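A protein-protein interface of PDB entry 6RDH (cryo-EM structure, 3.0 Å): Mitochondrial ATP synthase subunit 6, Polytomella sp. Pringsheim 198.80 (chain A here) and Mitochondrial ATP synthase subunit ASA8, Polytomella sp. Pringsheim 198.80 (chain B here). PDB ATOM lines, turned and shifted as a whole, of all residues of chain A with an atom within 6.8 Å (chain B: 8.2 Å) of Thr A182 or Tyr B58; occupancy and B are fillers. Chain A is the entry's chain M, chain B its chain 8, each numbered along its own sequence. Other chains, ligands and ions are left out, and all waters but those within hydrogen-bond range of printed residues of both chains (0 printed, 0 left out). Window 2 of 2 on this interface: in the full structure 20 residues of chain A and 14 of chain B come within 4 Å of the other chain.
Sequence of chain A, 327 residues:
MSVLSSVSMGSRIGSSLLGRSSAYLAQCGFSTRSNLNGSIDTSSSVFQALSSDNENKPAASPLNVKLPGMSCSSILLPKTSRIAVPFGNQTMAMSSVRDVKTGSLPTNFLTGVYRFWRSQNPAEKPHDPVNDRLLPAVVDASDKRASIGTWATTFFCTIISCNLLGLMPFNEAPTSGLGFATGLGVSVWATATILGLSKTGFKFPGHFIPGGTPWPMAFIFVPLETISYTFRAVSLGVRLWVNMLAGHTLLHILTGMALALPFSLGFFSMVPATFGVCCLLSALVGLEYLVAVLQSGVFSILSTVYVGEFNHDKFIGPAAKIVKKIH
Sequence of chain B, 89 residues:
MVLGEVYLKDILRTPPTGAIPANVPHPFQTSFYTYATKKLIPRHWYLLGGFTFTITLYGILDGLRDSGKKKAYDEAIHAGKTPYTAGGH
OG1 of Thr B54 sits close to N of Ser A187, at 3.3 Å.
The side-chain hydroxyl (OH) of Tyr B58 sits close to the backbone carbonyl oxygen (O) of Thr A182.
The backbone carbonyl oxygen (O) of Leu A184 sits at hydrogen-bond distance from the side-chain hydroxyl (OG) of Ser A187.
O of Gly A183 sits at hydrogen-bond distance from OG of Ser A187 (2.9 Å).
Gly A183 touches Thr B54 (O to CG2, 3.6 Å).
Tyr B58 touches Gly A183.
Val A186 touches Thr B54 (C to OG1, 3.7 Å).
Tyr B58 touches Val A186.
Phe B51 touches Ser A187.
Of the printed residues of chain B, Thr A182 touches Tyr B58 (3.3 Å).
Of the printed residues of chain A, Tyr B58 touches Thr A182, Gly A183 and Val A186.
Gly A183 touches just these residues of chain B: Thr B54 (3.6 Å) and Tyr B58 (3.7 Å).
Of the printed residues of chain A, Thr B54 touches Gly A183 (3.6 Å), Val A186 (3.7 Å) and Ser A187 (3.3 Å).
Printed residues of chain A within 4 Å of Phe B51: Ser A187 (3.3 Å).
Printed residues of chain B within 4 Å of Val A186: Thr B54 and Tyr B58.
Of the printed residues of chain B, Ser A187 touches Phe B51 (3.3 Å) and Thr B54 (3.3 Å).
Phe A180 touches none of the printed residues of chain B.
The nearest residue of chain B that does not touch Thr A182 is Thr B54 (5.0 Å).
The nearest printed residue of chain A that does not touch Tyr B58 is Gly A179 (4.1 Å).
Of the 15 printed residues of chain B, 3 touch a printed residue of chain A.
Of the 19 printed residues of chain A, 4 touch a printed residue of chain B.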
ATOM      1  N   THR A 175       1.060  31.663 -12.050  1.00  0.00           N
ATOM      2  CA  THR A 175       0.038  30.861 -12.701  1.00  0.00           C
ATOM      3  C   THR A 175      -0.945  31.688 -13.510  1.00  0.00           C
ATOM      4  O   THR A 175      -1.877  31.118 -14.074  1.00  0.00           O
ATOM      5  CB  THR A 175      -0.727  30.031 -11.678  1.00  0.00           C
ATOM      6  OG1 THR A 175      -1.081  30.864 -10.576  1.00  0.00           O
ATOM      7  CG2 THR A 175       0.107  28.890 -11.188  1.00  0.00           C
ATOM      8  N   GLY A 177       0.342  33.223 -16.013  1.00  0.00           N
ATOM      9  CA  GLY A 177       0.925  32.996 -17.313  1.00  0.00           C
ATOM     10  C   GLY A 177       0.274  31.789 -17.955  1.00  0.00           C
ATOM     11  O   GLY A 177      -0.098  30.832 -17.285  1.00  0.00           O
ATOM     12  N   LEU A 178       0.111  31.857 -19.272  1.00  0.00           N
ATOM     13  CA  LEU A 178      -0.540  30.770 -19.990  1.00  0.00           C
ATOM     14  C   LEU A 178       0.330  29.525 -20.002  1.00  0.00           C
ATOM     15  O   LEU A 178      -0.167  28.410 -19.800  1.00  0.00           O
ATOM     16  CB  LEU A 178      -0.866  31.221 -21.410  1.00  0.00           C
ATOM     17  CG  LEU A 178      -1.232  30.188 -22.466  1.00  0.00           C
ATOM     18  CD1 LEU A 178      -2.560  29.586 -22.154  1.00  0.00           C
ATOM     19  CD2 LEU A 178      -1.271  30.846 -23.811  1.00  0.00           C
ATOM     20  N   GLY A 179       1.635  29.703 -20.192  1.00  0.00           N
ATOM     21  CA  GLY A 179       2.522  28.563 -20.288  1.00  0.00           C
ATOM     22  C   GLY A 179       2.742  27.872 -18.960  1.00  0.00           C
ATOM     23  O   GLY A 179       2.804  26.649 -18.907  1.00  0.00           O
ATOM     24  N   PHE A 180       2.817  28.640 -17.871  1.00  0.00           N
ATOM     25  CA  PHE A 180       3.037  28.072 -16.544  1.00  0.00           C
ATOM     26  C   PHE A 180       1.865  27.207 -16.114  1.00  0.00           C
ATOM     27  O   PHE A 180       2.027  26.015 -15.827  1.00  0.00           O
ATOM     28  CB  PHE A 180       3.256  29.201 -15.541  1.00  0.00           C
ATOM     29  CG  PHE A 180       3.911  28.781 -14.255  1.00  0.00           C
ATOM     30  CD1 PHE A 180       5.245  29.036 -14.043  1.00  0.00           C
ATOM     31  CD2 PHE A 180       3.188  28.188 -13.239  1.00  0.00           C
ATOM     32  CE1 PHE A 180       5.845  28.678 -12.870  1.00  0.00           C
ATOM     33  CE2 PHE A 180       3.791  27.827 -12.072  1.00  0.00           C
ATOM     34  CZ  PHE A 180       5.119  28.070 -11.891  1.00  0.00           C
ATOM     35  N   ALA A 181       0.675  27.801 -16.060  1.00  0.00           N
ATOM     36  CA  ALA A 181      -0.507  27.094 -15.597  1.00  0.00           C
ATOM     37  C   ALA A 181      -0.904  25.985 -16.555  1.00  0.00           C
ATOM     38  O   ALA A 181      -1.216  24.864 -16.128  1.00  0.00           O
ATOM     39  CB  ALA A 181      -1.643  28.085 -15.416  1.00  0.00           C
ATOM     40  N   THR A 182      -0.848  26.259 -17.855  1.00  0.00           N
ATOM     41  CA  THR A 182      -1.223  25.239 -18.813  1.00  0.00           C
ATOM     42  C   THR A 182      -0.167  24.144 -18.893  1.00  0.00           C
ATOM     43  O   THR A 182      -0.497  22.996 -19.188  1.00  0.00           O
ATOM     44  CB  THR A 182      -1.464  25.883 -20.166  1.00  0.00           C
ATOM     45  OG1 THR A 182      -2.174  27.106 -19.971  1.00  0.00           O
ATOM     46  CG2 THR A 182      -2.365  25.003 -20.987  1.00  0.00           C
ATOM     47  N   GLY A 183       1.083  24.444 -18.543  1.00  0.00           N
ATOM     48  CA  GLY A 183       2.094  23.415 -18.494  1.00  0.00           C
ATOM     49  C   GLY A 183       1.964  22.523 -17.293  1.00  0.00           C
ATOM     50  O   GLY A 183       2.232  21.325 -17.387  1.00  0.00           O
ATOM     51  N   LEU A 184       1.537  23.077 -16.161  1.00  0.00           N
ATOM     52  CA  LEU A 184       1.212  22.240 -15.011  1.00  0.00           C
ATOM     53  C   LEU A 184       0.040  21.319 -15.319  1.00  0.00           C
ATOM     54  O   LEU A 184       0.066  20.135 -14.966  1.00  0.00           O
ATOM     55  CB  LEU A 184       0.906  23.109 -13.801  1.00  0.00           C
ATOM     56  CG  LEU A 184       2.107  23.798 -13.175  1.00  0.00           C
ATOM     57  CD1 LEU A 184       1.643  24.832 -12.194  1.00  0.00           C
ATOM     58  CD2 LEU A 184       2.967  22.792 -12.495  1.00  0.00           C
ATOM     59  N   GLY A 185      -0.973  21.828 -16.020  1.00  0.00           N
ATOM     60  CA  GLY A 185      -2.097  20.981 -16.395  1.00  0.00           C
ATOM     61  C   GLY A 185      -1.738  19.881 -17.381  1.00  0.00           C
ATOM     62  O   GLY A 185      -2.136  18.724 -17.206  1.00  0.00           O
ATOM     63  N   VAL A 186      -0.976  20.223 -18.423  1.00  0.00           N
ATOM     64  CA  VAL A 186      -0.561  19.232 -19.410  1.00  0.00           C
ATOM     65  C   VAL A 186       0.388  18.220 -18.787  1.00  0.00           C
ATOM     66  O   VAL A 186       0.332  17.034 -19.114  1.00  0.00           O
ATOM     67  CB  VAL A 186       0.051  19.941 -20.639  1.00  0.00           C
ATOM     68  CG1 VAL A 186       0.734  18.981 -21.578  1.00  0.00           C
ATOM     69  CG2 VAL A 186      -1.018  20.660 -21.403  1.00  0.00           C
ATOM     70  N   SER A 187       1.200  18.631 -17.819  1.00  0.00           N
ATOM     71  CA  SER A 187       2.098  17.675 -17.194  1.00  0.00           C
ATOM     72  C   SER A 187       1.388  16.744 -16.222  1.00  0.00           C
ATOM     73  O   SER A 187       1.795  15.587 -16.092  1.00  0.00           O
ATOM     74  CB  SER A 187       3.224  18.417 -16.503  1.00  0.00           C
ATOM     75  OG  SER A 187       2.728  19.208 -15.456  1.00  0.00           O
ATOM     76  N   ALA A 233      -6.305  17.542 -20.557  1.00  0.00           N
ATOM     77  CA  ALA A 233      -5.020  18.231 -20.605  1.00  0.00           C
ATOM     78  C   ALA A 233      -5.200  19.726 -20.768  1.00  0.00           C
ATOM     79  O   ALA A 233      -4.544  20.518 -20.085  1.00  0.00           O
ATOM     80  CB  ALA A 233      -4.182  17.702 -21.762  1.00  0.00           C
ATOM     81  N   VAL A 234      -6.078  20.131 -21.679  1.00  0.00           N
ATOM     82  CA  VAL A 234      -6.333  21.549 -21.881  1.00  0.00           C
ATOM     83  C   VAL A 234      -7.119  22.111 -20.711  1.00  0.00           C
ATOM     84  O   VAL A 234      -6.809  23.191 -20.204  1.00  0.00           O
ATOM     85  CB  VAL A 234      -7.066  21.775 -23.211  1.00  0.00           C
ATOM     86  CG1 VAL A 234      -7.144  23.246 -23.521  1.00  0.00           C
ATOM     87  CG2 VAL A 234      -6.372  21.026 -24.321  1.00  0.00           C
ATOM     88  N   LEU A 236      -7.607  21.141 -17.482  1.00  0.00           N
ATOM     89  CA  LEU A 236      -7.003  21.190 -16.156  1.00  0.00           C
ATOM     90  C   LEU A 236      -6.045  22.361 -16.015  1.00  0.00           C
ATOM     91  O   LEU A 236      -5.958  22.973 -14.949  1.00  0.00           O
ATOM     92  CB  LEU A 236      -6.279  19.879 -15.889  1.00  0.00           C
ATOM     93  CG  LEU A 236      -5.720  19.650 -14.502  1.00  0.00           C
ATOM     94  CD1 LEU A 236      -6.810  19.780 -13.504  1.00  0.00           C
ATOM     95  CD2 LEU A 236      -5.177  18.287 -14.465  1.00  0.00           C
ATOM     96  N   GLY A 237      -5.334  22.696 -17.079  1.00  0.00           N
ATOM     97  CA  GLY A 237      -4.462  23.843 -17.040  1.00  0.00           C
ATOM     98  C   GLY A 237      -5.195  25.149 -17.236  1.00  0.00           C
ATOM     99  O   GLY A 237      -4.975  26.101 -16.481  1.00  0.00           O
ATOM    100  N   VAL A 238      -6.072  25.233 -18.240  1.00  0.00           N
ATOM    101  CA  VAL A 238      -6.657  26.536 -18.523  1.00  0.00           C
ATOM    102  C   VAL A 238      -7.776  26.909 -17.574  1.00  0.00           C
ATOM    103  O   VAL A 238      -8.136  28.081 -17.535  1.00  0.00           O
ATOM    104  CB  VAL A 238      -7.190  26.705 -19.957  1.00  0.00           C
ATOM    105  CG1 VAL A 238      -6.155  26.275 -20.959  1.00  0.00           C
ATOM    106  CG2 VAL A 238      -8.485  25.984 -20.149  1.00  0.00           C
ATOM    107  N   LEU A 240      -7.205  26.796 -14.307  1.00  0.00           N
ATOM    108  CA  LEU A 240      -6.320  27.535 -13.415  1.00  0.00           C
ATOM    109  C   LEU A 240      -5.856  28.839 -14.043  1.00  0.00           C
ATOM    110  O   LEU A 240      -5.859  29.887 -13.386  1.00  0.00           O
ATOM    111  CB  LEU A 240      -5.127  26.654 -13.064  1.00  0.00           C
ATOM    112  CG  LEU A 240      -3.971  27.226 -12.270  1.00  0.00           C
ATOM    113  CD1 LEU A 240      -4.403  27.512 -10.862  1.00  0.00           C
ATOM    114  CD2 LEU A 240      -2.840  26.238 -12.283  1.00  0.00           C
ATOM    115  N   TRP A 241      -5.493  28.801 -15.328  1.00  0.00           N
ATOM    116  CA  TRP A 241      -4.989  29.999 -15.994  1.00  0.00           C
ATOM    117  C   TRP A 241      -6.068  31.060 -16.151  1.00  0.00           C
ATOM    118  O   TRP A 241      -5.823  32.239 -15.880  1.00  0.00           O
ATOM    119  CB  TRP A 241      -4.414  29.661 -17.356  1.00  0.00           C
ATOM    120  CG  TRP A 241      -4.110  30.882 -18.131  1.00  0.00           C
ATOM    121  CD1 TRP A 241      -3.290  31.893 -17.761  1.00  0.00           C
ATOM    122  CD2 TRP A 241      -4.632  31.239 -19.408  1.00  0.00           C
ATOM    123  NE1 TRP A 241      -3.262  32.862 -18.725  1.00  0.00           N
ATOM    124  CE2 TRP A 241      -4.081  32.481 -19.751  1.00  0.00           C
ATOM    125  CE3 TRP A 241      -5.513  30.628 -20.298  1.00  0.00           C
ATOM    126  CZ2 TRP A 241      -4.376  33.119 -20.939  1.00  0.00           C
ATOM    127  CZ3 TRP A 241      -5.807  31.265 -21.469  1.00  0.00           C
ATOM    128  CH2 TRP A 241      -5.240  32.498 -21.784  1.00  0.00           C
ATOM    129  N   PHE B  51       6.664  16.098 -17.205  1.00  0.00           N
ATOM    130  CA  PHE B  51       7.322  17.388 -17.368  1.00  0.00           C
ATOM    131  C   PHE B  51       8.124  17.442 -18.660  1.00  0.00           C
ATOM    132  O   PHE B  51       8.112  18.464 -19.354  1.00  0.00           O
ATOM    133  CB  PHE B  51       8.214  17.678 -16.166  1.00  0.00           C
ATOM    134  CG  PHE B  51       7.455  18.044 -14.932  1.00  0.00           C
ATOM    135  CD1 PHE B  51       6.387  18.907 -15.001  1.00  0.00           C
ATOM    136  CD2 PHE B  51       7.800  17.521 -13.707  1.00  0.00           C
ATOM    137  CE1 PHE B  51       5.673  19.238 -13.877  1.00  0.00           C
ATOM    138  CE2 PHE B  51       7.092  17.847 -12.583  1.00  0.00           C
ATOM    139  CZ  PHE B  51       6.028  18.706 -12.671  1.00  0.00           C
ATOM    140  N   THR B  52       8.786  16.345 -19.031  1.00  0.00           N
ATOM    141  CA  THR B  52       9.504  16.349 -20.300  1.00  0.00           C
ATOM    142  C   THR B  52       8.564  16.333 -21.492  1.00  0.00           C
ATOM    143  O   THR B  52       8.880  16.947 -22.518  1.00  0.00           O
ATOM    144  CB  THR B  52      10.466  15.177 -20.394  1.00  0.00           C
ATOM    145  OG1 THR B  52       9.752  13.956 -20.191  1.00  0.00           O
ATOM    146  CG2 THR B  52      11.570  15.322 -19.375  1.00  0.00           C
ATOM    147  N   PHE B  53       7.414  15.661 -21.385  1.00  0.00           N
ATOM    148  CA  PHE B  53       6.431  15.715 -22.459  1.00  0.00           C
ATOM    149  C   PHE B  53       5.914  17.127 -22.656  1.00  0.00           C
ATOM    150  O   PHE B  53       5.762  17.579 -23.793  1.00  0.00           O
ATOM    151  CB  PHE B  53       5.263  14.778 -22.177  1.00  0.00           C
ATOM    152  CG  PHE B  53       4.139  14.904 -23.167  1.00  0.00           C
ATOM    153  CD1 PHE B  53       4.244  14.336 -24.416  1.00  0.00           C
ATOM    154  CD2 PHE B  53       2.980  15.591 -22.852  1.00  0.00           C
ATOM    155  CE1 PHE B  53       3.226  14.451 -25.327  1.00  0.00           C
ATOM    156  CE2 PHE B  53       1.961  15.707 -23.762  1.00  0.00           C
ATOM    157  CZ  PHE B  53       2.085  15.136 -24.997  1.00  0.00           C
ATOM    158  N   THR B  54       5.644  17.838 -21.564  1.00  0.00           N
ATOM    159  CA  THR B  54       5.152  19.201 -21.694  1.00  0.00           C
ATOM    160  C   THR B  54       6.212  20.126 -22.267  1.00  0.00           C
ATOM    161  O   THR B  54       5.897  20.993 -23.085  1.00  0.00           O
ATOM    162  CB  THR B  54       4.680  19.717 -20.351  1.00  0.00           C
ATOM    163  OG1 THR B  54       3.915  18.696 -19.722  1.00  0.00           O
ATOM    164  CG2 THR B  54       3.810  20.898 -20.540  1.00  0.00           C
ATOM    165  N   ILE B  55       7.474  19.939 -21.884  1.00  0.00           N
ATOM    166  CA  ILE B  55       8.525  20.805 -22.405  1.00  0.00           C
ATOM    167  C   ILE B  55       8.756  20.551 -23.895  1.00  0.00           C
ATOM    168  O   ILE B  55       8.902  21.498 -24.677  1.00  0.00           O
ATOM    169  CB  ILE B  55       9.797  20.633 -21.565  1.00  0.00           C
ATOM    170  CG1 ILE B  55       9.560  21.226 -20.189  1.00  0.00           C
ATOM    171  CG2 ILE B  55      10.962  21.338 -22.184  1.00  0.00           C
ATOM    172  CD1 ILE B  55      10.559  20.804 -19.176  1.00  0.00           C
ATOM    173  N   THR B  56       8.696  19.288 -24.332  1.00  0.00           N
ATOM    174  CA  THR B  56       8.840  19.017 -25.762  1.00  0.00           C
ATOM    175  C   THR B  56       7.625  19.480 -26.557  1.00  0.00           C
ATOM    176  O   THR B  56       7.777  20.001 -27.666  1.00  0.00           O
ATOM    177  CB  THR B  56       9.090  17.539 -26.015  1.00  0.00           C
ATOM    178  OG1 THR B  56       8.012  16.775 -25.477  1.00  0.00           O
ATOM    179  CG2 THR B  56      10.391  17.109 -25.385  1.00  0.00           C
ATOM    180  N   LEU B  57       6.419  19.330 -26.005  1.00  0.00           N
ATOM    181  CA  LEU B  57       5.219  19.780 -26.702  1.00  0.00           C
ATOM    182  C   LEU B  57       5.188  21.295 -26.835  1.00  0.00           C
ATOM    183  O   LEU B  57       4.779  21.829 -27.871  1.00  0.00           O
ATOM    184  CB  LEU B  57       3.981  19.292 -25.963  1.00  0.00           C
ATOM    185  CG  LEU B  57       2.643  19.726 -26.544  1.00  0.00           C
ATOM    186  CD1 LEU B  57       2.374  18.969 -27.823  1.00  0.00           C
ATOM    187  CD2 LEU B  57       1.535  19.523 -25.545  1.00  0.00           C
ATOM    188  N   TYR B  58       5.653  22.007 -25.824  1.00  0.00           N
ATOM    189  CA  TYR B  58       5.643  23.452 -25.928  1.00  0.00           C
ATOM    190  C   TYR B  58       6.801  23.954 -26.765  1.00  0.00           C
ATOM    191  O   TYR B  58       6.698  25.032 -27.352  1.00  0.00           O
ATOM    192  CB  TYR B  58       5.646  24.078 -24.540  1.00  0.00           C
ATOM    193  CG  TYR B  58       4.277  24.132 -23.905  1.00  0.00           C
ATOM    194  CD1 TYR B  58       3.531  22.989 -23.719  1.00  0.00           C
ATOM    195  CD2 TYR B  58       3.737  25.324 -23.487  1.00  0.00           C
ATOM    196  CE1 TYR B  58       2.308  23.026 -23.156  1.00  0.00           C
ATOM    197  CE2 TYR B  58       2.500  25.369 -22.917  1.00  0.00           C
ATOM    198  CZ  TYR B  58       1.799  24.213 -22.757  1.00  0.00           C
ATOM    199  OH  TYR B  58       0.569  24.234 -22.187  1.00  0.00           O
ATOM    200  N   GLY B  59       7.873  23.169 -26.886  1.00  0.00           N
ATOM    201  CA  GLY B  59       8.871  23.462 -27.899  1.00  0.00           C
ATOM    202  C   GLY B  59       8.330  23.289 -29.301  1.00  0.00           C
ATOM    203  O   GLY B  59       8.656  24.071 -30.198  1.00  0.00           O
ATOM    204  N   ILE B  60       7.481  22.277 -29.503  1.00  0.00           N
ATOM    205  CA  ILE B  60       6.801  22.085 -30.786  1.00  0.00           C
ATOM    206  C   ILE B  60       5.900  23.277 -31.102  1.00  0.00           C
ATOM    207  O   ILE B  60       5.908  23.798 -32.222  1.00  0.00           O
ATOM    208  CB  ILE B  60       6.006  20.765 -30.777  1.00  0.00           C
ATOM    209  CG1 ILE B  60       6.928  19.556 -30.746  1.00  0.00           C
ATOM    210  CG2 ILE B  60       5.106  20.658 -31.971  1.00  0.00           C
ATOM    211  CD1 ILE B  60       7.950  19.553 -31.810  1.00  0.00           C
ATOM    212  N   LEU B  61       5.142  23.747 -30.111  1.00  0.00           N
ATOM    213  CA  LEU B  61       4.253  24.888 -30.330  1.00  0.00           C
ATOM    214  C   LEU B  61       5.029  26.181 -30.557  1.00  0.00           C
ATOM    215  O   LEU B  61       4.600  27.038 -31.340  1.00  0.00           O
ATOM    216  CB  LEU B  61       3.301  25.052 -29.152  1.00  0.00           C
ATOM    217  CG  LEU B  61       2.329  23.918 -28.859  1.00  0.00           C
ATOM    218  CD1 LEU B  61       1.336  24.352 -27.805  1.00  0.00           C
ATOM    219  CD2 LEU B  61       1.627  23.480 -30.115  1.00  0.00           C
ATOM    220  N   ASP B  62       6.179  26.342 -29.902  1.00  0.00           N
ATOM    221  CA  ASP B  62       7.025  27.500 -30.172  1.00  0.00           C
ATOM    222  C   ASP B  62       7.621  27.440 -31.572  1.00  0.00           C
ATOM    223  O   ASP B  62       7.788  28.476 -32.226  1.00  0.00           O
ATOM    224  CB  ASP B  62       8.136  27.588 -29.132  1.00  0.00           C
ATOM    225  CG  ASP B  62       7.707  28.313 -27.885  1.00  0.00           C
ATOM    226  OD1 ASP B  62       6.748  29.104 -27.956  1.00  0.00           O
ATOM    227  OD2 ASP B  62       8.344  28.102 -26.833  1.00  0.00           O
ATOM    228  N   GLY B  63       7.946  26.235 -32.044  1.00  0.00           N
ATOM    229  CA  GLY B  63       8.413  26.089 -33.410  1.00  0.00           C
ATOM    230  C   GLY B  63       7.340  26.415 -34.427  1.00  0.00           C
ATOM    231  O   GLY B  63       7.616  27.055 -35.445  1.00  0.00           O
ATOM    232  N   LEU B  64       6.097  26.015 -34.145  1.00  0.00           N
ATOM    233  CA  LEU B  64       4.981  26.375 -35.018  1.00  0.00           C
ATOM    234  C   LEU B  64       4.761  27.879 -35.035  1.00  0.00           C
ATOM    235  O   LEU B  64       4.515  28.464 -36.097  1.00  0.00           O
ATOM    236  CB  LEU B  64       3.700  25.676 -34.579  1.00  0.00           C
ATOM    237  CG  LEU B  64       3.633  24.154 -34.608  1.00  0.00           C
ATOM    238  CD1 LEU B  64       2.215  23.714 -34.382  1.00  0.00           C
ATOM    239  CD2 LEU B  64       4.166  23.603 -35.899  1.00  0.00           C
ATOM    240  N   ARG B  65       4.898  28.528 -33.880  1.00  0.00           N
ATOM    241  CA  ARG B  65       4.653  29.963 -33.821  1.00  0.00           C
ATOM    242  C   ARG B  65       5.743  30.760 -34.525  1.00  0.00           C
ATOM    243  O   ARG B  65       5.441  31.717 -35.249  1.00  0.00           O
ATOM    244  CB  ARG B  65       4.523  30.415 -32.377  1.00  0.00           C
ATOM    245  CG  ARG B  65       3.956  31.793 -32.251  1.00  0.00           C
ATOM    246  CD  ARG B  65       3.055  31.881 -31.054  1.00  0.00           C
ATOM    247  NE  ARG B  65       3.728  31.401 -29.859  1.00  0.00           N
ATOM    248  CZ  ARG B  65       4.349  32.194 -28.998  1.00  0.00           C
ATOM    249  NH1 ARG B  65       4.940  31.679 -27.936  1.00  0.00           N
ATOM    250  NH2 ARG B  65       4.373  33.501 -29.202  1.00  0.00           N
